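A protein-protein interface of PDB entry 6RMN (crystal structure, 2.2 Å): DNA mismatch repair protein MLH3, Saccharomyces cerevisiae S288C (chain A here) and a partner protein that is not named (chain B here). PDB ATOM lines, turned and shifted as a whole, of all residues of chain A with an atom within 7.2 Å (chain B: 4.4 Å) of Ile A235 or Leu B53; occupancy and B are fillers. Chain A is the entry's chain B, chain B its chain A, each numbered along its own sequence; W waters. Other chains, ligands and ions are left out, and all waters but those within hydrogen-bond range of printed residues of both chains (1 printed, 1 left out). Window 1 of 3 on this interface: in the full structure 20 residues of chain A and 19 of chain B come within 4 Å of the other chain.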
ATOM      1  N   VAL A  23     -21.343  22.147  29.399  1.00  0.00           N
ATOM      2  CA  VAL A  23     -21.219  21.388  28.155  1.00  0.00           C
ATOM      3  C   VAL A  23     -21.471  22.342  26.984  1.00  0.00           C
ATOM      4  O   VAL A  23     -22.531  22.965  26.930  1.00  0.00           O
ATOM      5  CB  VAL A  23     -22.229  20.194  28.132  1.00  0.00           C
ATOM      6  CG1 VAL A  23     -22.315  19.547  26.750  1.00  0.00           C
ATOM      7  CG2 VAL A  23     -21.892  19.155  29.189  1.00  0.00           C
ATOM      8  N   ASP A  24     -20.494  22.451  26.056  1.00  0.00           N
ATOM      9  CA  ASP A  24     -20.542  23.216  24.798  1.00  0.00           C
ATOM     10  C   ASP A  24     -20.850  24.720  24.976  1.00  0.00           C
ATOM     11  O   ASP A  24     -21.248  25.380  24.013  1.00  0.00           O
ATOM     12  CB  ASP A  24     -21.549  22.538  23.831  1.00  0.00           C
ATOM     13  CG  ASP A  24     -21.495  22.982  22.384  1.00  0.00           C
ATOM     14  OD1 ASP A  24     -20.400  22.923  21.783  1.00  0.00           O
ATOM     15  OD2 ASP A  24     -22.550  23.377  21.848  1.00  0.00           O
ATOM     16  N   LEU A  29     -24.616  20.081  32.575  1.00  0.00           N
ATOM     17  CA  LEU A  29     -24.892  18.656  32.727  1.00  0.00           C
ATOM     18  C   LEU A  29     -25.051  18.330  34.208  1.00  0.00           C
ATOM     19  O   LEU A  29     -24.185  18.668  35.024  1.00  0.00           O
ATOM     20  CB  LEU A  29     -23.802  17.783  32.074  1.00  0.00           C
ATOM     21  CG  LEU A  29     -23.963  16.235  32.155  1.00  0.00           C
ATOM     22  CD1 LEU A  29     -25.169  15.733  31.326  1.00  0.00           C
ATOM     23  CD2 LEU A  29     -22.670  15.528  31.700  1.00  0.00           C
ATOM     24  N   ILE A  30     -26.194  17.711  34.548  1.00  0.00           N
ATOM     25  CA  ILE A  30     -26.531  17.320  35.915  1.00  0.00           C
ATOM     26  C   ILE A  30     -26.859  15.822  35.996  1.00  0.00           C
ATOM     27  O   ILE A  30     -27.331  15.224  35.022  1.00  0.00           O
ATOM     28  CB  ILE A  30     -27.629  18.237  36.544  1.00  0.00           C
ATOM     29  CG1 ILE A  30     -29.003  18.114  35.820  1.00  0.00           C
ATOM     30  CG2 ILE A  30     -27.155  19.716  36.621  1.00  0.00           C
ATOM     31  CD1 ILE A  30     -30.257  18.721  36.581  1.00  0.00           C
ATOM     32  N   LEU A  42     -31.674  10.026  35.091  1.00  0.00           N
ATOM     33  CA  LEU A  42     -30.302  10.011  35.613  1.00  0.00           C
ATOM     34  C   LEU A  42     -29.458  11.202  35.112  1.00  0.00           C
ATOM     35  O   LEU A  42     -28.882  11.898  35.940  1.00  0.00           O
ATOM     36  CB  LEU A  42     -29.585   8.659  35.359  1.00  0.00           C
ATOM     37  CG  LEU A  42     -28.082   8.563  35.795  1.00  0.00           C
ATOM     38  CD1 LEU A  42     -27.930   7.893  37.161  1.00  0.00           C
ATOM     39  CD2 LEU A  42     -27.229   7.836  34.746  1.00  0.00           C
ATOM     40  N   LEU A  43     -29.356  11.418  33.783  1.00  0.00           N
ATOM     41  CA  LEU A  43     -28.585  12.527  33.202  1.00  0.00           C
ATOM     42  C   LEU A  43     -29.492  13.553  32.533  1.00  0.00           C
ATOM     43  O   LEU A  43     -30.342  13.195  31.710  1.00  0.00           O
ATOM     44  CB  LEU A  43     -27.491  12.048  32.216  1.00  0.00           C
ATOM     45  CG  LEU A  43     -26.209  11.378  32.772  1.00  0.00           C
ATOM     46  CD1 LEU A  43     -25.216  11.121  31.654  1.00  0.00           C
ATOM     47  CD2 LEU A  43     -25.511  12.227  33.832  1.00  0.00           C
ATOM     48  N   VAL A  44     -29.314  14.833  32.893  1.00  0.00           N
ATOM     49  CA  VAL A  44     -30.103  15.952  32.373  1.00  0.00           C
ATOM     50  C   VAL A  44     -29.179  17.109  31.927  1.00  0.00           C
ATOM     51  O   VAL A  44     -28.200  17.427  32.616  1.00  0.00           O
ATOM     52  CB  VAL A  44     -31.164  16.415  33.429  1.00  0.00           C
ATOM     53  CG1 VAL A  44     -31.819  17.750  33.063  1.00  0.00           C
ATOM     54  CG2 VAL A  44     -32.228  15.345  33.673  1.00  0.00           C
ATOM     55  N   LEU A  45     -29.517  17.735  30.767  1.00  0.00           N
ATOM     56  CA  LEU A  45     -28.856  18.925  30.219  1.00  0.00           C
ATOM     57  C   LEU A  45     -29.793  20.146  30.417  1.00  0.00           C
ATOM     58  O   LEU A  45     -30.921  20.170  29.902  1.00  0.00           O
ATOM     59  CB  LEU A  45     -28.499  18.752  28.732  1.00  0.00           C
ATOM     60  CG  LEU A  45     -27.309  17.848  28.397  1.00  0.00           C
ATOM     61  CD1 LEU A  45     -27.235  17.592  26.899  1.00  0.00           C
ATOM     62  CD2 LEU A  45     -26.000  18.455  28.863  1.00  0.00           C
ATOM     63  N   VAL A 233     -33.665  19.032  29.464  1.00  0.00           N
ATOM     64  CA  VAL A 233     -33.973  17.830  28.688  1.00  0.00           C
ATOM     65  C   VAL A 233     -33.240  16.619  29.285  1.00  0.00           C
ATOM     66  O   VAL A 233     -32.023  16.682  29.489  1.00  0.00           O
ATOM     67  CB  VAL A 233     -33.660  18.034  27.169  1.00  0.00           C
ATOM     68  CG1 VAL A 233     -33.660  16.721  26.400  1.00  0.00           C
ATOM     69  CG2 VAL A 233     -34.647  19.000  26.531  1.00  0.00           C
ATOM     70  N   PRO A 234     -33.957  15.513  29.584  1.00  0.00           N
ATOM     71  CA  PRO A 234     -33.249  14.316  30.069  1.00  0.00           C
ATOM     72  C   PRO A 234     -32.538  13.670  28.878  1.00  0.00           C
ATOM     73  O   PRO A 234     -33.093  13.631  27.773  1.00  0.00           O
ATOM     74  CB  PRO A 234     -34.363  13.431  30.628  1.00  0.00           C
ATOM     75  CG  PRO A 234     -35.621  13.867  29.915  1.00  0.00           C
ATOM     76  CD  PRO A 234     -35.406  15.262  29.379  1.00  0.00           C
ATOM     77  N   ILE A 235     -31.292  13.231  29.068  1.00  0.00           N
ATOM     78  CA  ILE A 235     -30.559  12.622  27.960  1.00  0.00           C
ATOM     79  C   ILE A 235     -30.260  11.131  28.220  1.00  0.00           C
ATOM     80  O   ILE A 235     -29.925  10.409  27.277  1.00  0.00           O
ATOM     81  CB  ILE A 235     -29.299  13.437  27.545  1.00  0.00           C
ATOM     82  CG1 ILE A 235     -28.299  13.616  28.708  1.00  0.00           C
ATOM     83  CG2 ILE A 235     -29.707  14.774  26.918  1.00  0.00           C
ATOM     84  CD1 ILE A 235     -26.891  13.825  28.278  1.00  0.00           C
ATOM     85  N   ALA A 236     -30.413  10.674  29.482  1.00  0.00           N
ATOM     86  CA  ALA A 236     -30.155   9.289  29.896  1.00  0.00           C
ATOM     87  C   ALA A 236     -31.141   8.299  29.262  1.00  0.00           C
ATOM     88  O   ALA A 236     -30.931   7.839  28.139  1.00  0.00           O
ATOM     89  CB  ALA A 236     -30.203   9.179  31.411  1.00  0.00           C
ATOM     90  N   VAL B  35     -15.582  16.474  30.156  1.00  0.00           N
ATOM     91  CA  VAL B  35     -16.667  17.134  30.894  1.00  0.00           C
ATOM     92  C   VAL B  35     -16.567  16.871  32.417  1.00  0.00           C
ATOM     93  O   VAL B  35     -16.476  17.830  33.187  1.00  0.00           O
ATOM     94  CB  VAL B  35     -18.088  16.823  30.329  1.00  0.00           C
ATOM     95  CG1 VAL B  35     -19.165  17.595  31.099  1.00  0.00           C
ATOM     96  CG2 VAL B  35     -18.177  17.118  28.827  1.00  0.00           C
ATOM     97  N   ILE B  47     -17.508  12.871  28.142  1.00  0.00           N
ATOM     98  CA  ILE B  47     -16.621  13.632  27.261  1.00  0.00           C
ATOM     99  C   ILE B  47     -17.455  14.122  26.079  1.00  0.00           C
ATOM    100  O   ILE B  47     -18.519  13.559  25.782  1.00  0.00           O
ATOM    101  CB  ILE B  47     -15.362  12.841  26.750  1.00  0.00           C
ATOM    102  CG1 ILE B  47     -15.760  11.663  25.819  1.00  0.00           C
ATOM    103  CG2 ILE B  47     -14.431  12.390  27.889  1.00  0.00           C
ATOM    104  CD1 ILE B  47     -15.019  11.567  24.533  1.00  0.00           C
ATOM    105  N   GLN B  48     -16.953  15.156  25.394  1.00  0.00           N
ATOM    106  CA  GLN B  48     -17.554  15.665  24.177  1.00  0.00           C
ATOM    107  C   GLN B  48     -16.556  15.441  23.047  1.00  0.00           C
ATOM    108  O   GLN B  48     -15.369  15.740  23.204  1.00  0.00           O
ATOM    109  CB  GLN B  48     -17.901  17.163  24.303  1.00  0.00           C
ATOM    110  CG  GLN B  48     -18.660  17.710  23.098  1.00  0.00           C
ATOM    111  CD  GLN B  48     -18.988  19.180  23.177  1.00  0.00           C
ATOM    112  OE1 GLN B  48     -19.157  19.762  24.252  1.00  0.00           O
ATOM    113  NE2 GLN B  48     -19.113  19.809  22.026  1.00  0.00           N
ATOM    114  N   LYS B  52     -21.049  15.842  19.822  1.00  0.00           N
ATOM    115  CA  LYS B  52     -21.643  14.641  20.402  1.00  0.00           C
ATOM    116  C   LYS B  52     -21.121  14.441  21.808  1.00  0.00           C
ATOM    117  O   LYS B  52     -19.949  14.718  22.076  1.00  0.00           O
ATOM    118  CB  LYS B  52     -21.314  13.404  19.557  1.00  0.00           C
ATOM    119  CG  LYS B  52     -22.279  13.164  18.416  1.00  0.00           C
ATOM    120  CD  LYS B  52     -22.020  11.840  17.725  1.00  0.00           C
ATOM    121  CE  LYS B  52     -22.704  11.777  16.384  1.00  0.00           C
ATOM    122  NZ  LYS B  52     -22.010  12.618  15.375  1.00  0.00           N
ATOM    123  N   LEU B  53     -21.995  13.957  22.699  1.00  0.00           N
ATOM    124  CA  LEU B  53     -21.668  13.665  24.090  1.00  0.00           C
ATOM    125  C   LEU B  53     -21.582  12.150  24.295  1.00  0.00           C
ATOM    126  O   LEU B  53     -22.457  11.399  23.832  1.00  0.00           O
ATOM    127  CB  LEU B  53     -22.703  14.291  25.024  1.00  0.00           C
ATOM    128  CG  LEU B  53     -22.212  14.716  26.402  1.00  0.00           C
ATOM    129  CD1 LEU B  53     -21.224  15.873  26.295  1.00  0.00           C
ATOM    130  CD2 LEU B  53     -23.395  15.143  27.269  1.00  0.00           C
ATOM    131  N   PHE B  54     -20.490  11.707  24.953  1.00  0.00           N
ATOM    132  CA  PHE B  54     -20.214  10.301  25.196  1.00  0.00           C
ATOM    133  C   PHE B  54     -20.060   9.939  26.662  1.00  0.00           C
ATOM    134  O   PHE B  54     -19.533  10.723  27.455  1.00  0.00           O
ATOM    135  CB  PHE B  54     -18.951   9.847  24.427  1.00  0.00           C
ATOM    136  CG  PHE B  54     -19.074   9.848  22.922  1.00  0.00           C
ATOM    137  CD1 PHE B  54     -19.501   8.711  22.242  1.00  0.00           C
ATOM    138  CD2 PHE B  54     -18.768  10.989  22.182  1.00  0.00           C
ATOM    139  CE1 PHE B  54     -19.630   8.718  20.847  1.00  0.00           C
ATOM    140  CE2 PHE B  54     -18.892  10.993  20.789  1.00  0.00           C
ATOM    141  CZ  PHE B  54     -19.322   9.859  20.131  1.00  0.00           C
ATOM    142  N   VAL B 250     -20.168   4.934  24.673  1.00  0.00           N
ATOM    143  CA  VAL B 250     -21.574   5.085  24.271  1.00  0.00           C
ATOM    144  C   VAL B 250     -21.961   6.550  24.006  1.00  0.00           C
ATOM    145  O   VAL B 250     -21.727   7.407  24.861  1.00  0.00           O
ATOM    146  CB  VAL B 250     -22.542   4.444  25.323  1.00  0.00           C
ATOM    147  CG1 VAL B 250     -23.952   4.292  24.762  1.00  0.00           C
ATOM    148  CG2 VAL B 250     -22.024   3.104  25.838  1.00  0.00           C
ATOM    149  N   GLU B 251     -22.625   6.811  22.859  1.00  0.00           N
ATOM    150  CA  GLU B 251     -23.134   8.133  22.506  1.00  0.00           C
ATOM    151  C   GLU B 251     -24.422   8.376  23.315  1.00  0.00           C
ATOM    152  O   GLU B 251     -25.404   7.664  23.115  1.00  0.00           O
ATOM    153  CB  GLU B 251     -23.403   8.235  20.989  1.00  0.00           C
ATOM    154  CG  GLU B 251     -23.640   9.659  20.505  1.00  0.00           C
ATOM    155  CD  GLU B 251     -24.805   9.847  19.551  1.00  0.00           C
ATOM    156  OE1 GLU B 251     -25.849  10.391  19.982  1.00  0.00           O
ATOM    157  OE2 GLU B 251     -24.671   9.459  18.366  1.00  0.00           O
ATOM    158  N   ILE B 252     -24.407   9.360  24.241  1.00  0.00           N
ATOM    159  CA  ILE B 252     -25.562   9.692  25.090  1.00  0.00           C
ATOM    160  C   ILE B 252     -26.392  10.878  24.541  1.00  0.00           C
ATOM    161  O   ILE B 252     -27.602  10.931  24.788  1.00  0.00           O
ATOM    162  CB  ILE B 252     -25.190   9.882  26.580  1.00  0.00           C
ATOM    163  CG1 ILE B 252     -23.964  10.825  26.760  1.00  0.00           C
ATOM    164  CG2 ILE B 252     -24.983   8.523  27.232  1.00  0.00           C
ATOM    165  CD1 ILE B 252     -23.738  11.396  28.165  1.00  0.00           C
ATOM    166  N   ALA B 253     -25.760  11.804  23.783  1.00  0.00           N
ATOM    167  CA  ALA B 253     -26.447  12.949  23.189  1.00  0.00           C
ATOM    168  C   ALA B 253     -25.796  13.446  21.902  1.00  0.00           C
ATOM    169  O   ALA B 253     -24.570  13.448  21.785  1.00  0.00           O
ATOM    170  CB  ALA B 253     -26.535  14.090  24.189  1.00  0.00           C
HETATM  171  O   HOH W   1     -18.216  20.616  26.631  1.00  0.00           O
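N of Ile B252 lies within hydrogen-bond range of O of Leu B53, 2.9 Å away.
The backbone NH (N) of Leu B53 is in hydrogen-bond range of the backbone carbonyl oxygen (O) of Ala B253 (2.8 Å).
The backbone carbonyl oxygen (O) of Leu A43 sits at hydrogen-bond distance from the backbone NH (N) of Ile A235, 2.8 Å away.
The backbone carbonyl oxygen of Leu A43 is in hydrogen-bond range of the backbone NH of Ala A236 (3.4 Å).
Of the printed residues of chain B, Val A23 touches Val B35 (3.7 Å) and Leu B53 (3.9 Å).
Of the printed residues of chain B, Asp A24 touches Gln B48.
Of the printed residues of chain B, Leu A43 touches Ile B252.
Ile A235 touches just these residues of chain B: Leu B53 and Ile B252.
Printed residues of chain A within 4 Å of Gln B48: Asp A24.
Of chain A, only Val A23 (3.9 Å) and Ile A235 (3.9 Å) come within 4 Å of Leu B53.
Of the printed residues of chain A, Ile B252 touches Leu A43 (3.8 Å) and Ile A235 (3.4 Å).
The nearest residue of chain B that does not touch Ile A235 is Ala B253 (4.1 Å).
The nearest printed residue of chain A that does not touch Ile B252 is Ala A236 (5.5 Å).
Printed residues of chain B that touch a printed residue of chain A: Val B35, Gln B48, Leu B53 and Ile B252.
Of the 12 printed residues of chain A, 4 touch a printed residue of chain B.
Hydrophobic or aromatic side chains of chain A within 4 Å of the printed part of chain B: Val A23, Leu A43 and Ile A235.
Among the printed residues, 6 pairs touch across the chains.
Among the printed residues, no Asp or Glu carboxylate lies within 4 Å of a Lys or Arg side-chain nitrogen of the other chain.
Water W1 lies within hydrogen-bond range of the side-chain amide oxygen (OE1) of Gln B48 and the backbone NH (N) of Asp A24.
The side-chain amide nitrogen of Gln B48 lies within hydrogen-bond range of the side-chain carboxylate of Asp A24 (3.4 Å).
The backbone carbonyl oxygen of Ile A235 sits close to the backbone carbonyl oxygen of Ile B252 (3.4 Å).
Among the printed residues, merely in contact across the chains: Val A23 with Val B35 (3.7 Å), Leu A43 with Ile B252 (3.8 Å), Val A23 with Leu B53 (3.9 Å) and Ile A235 with Leu B53 (3.9 Å).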
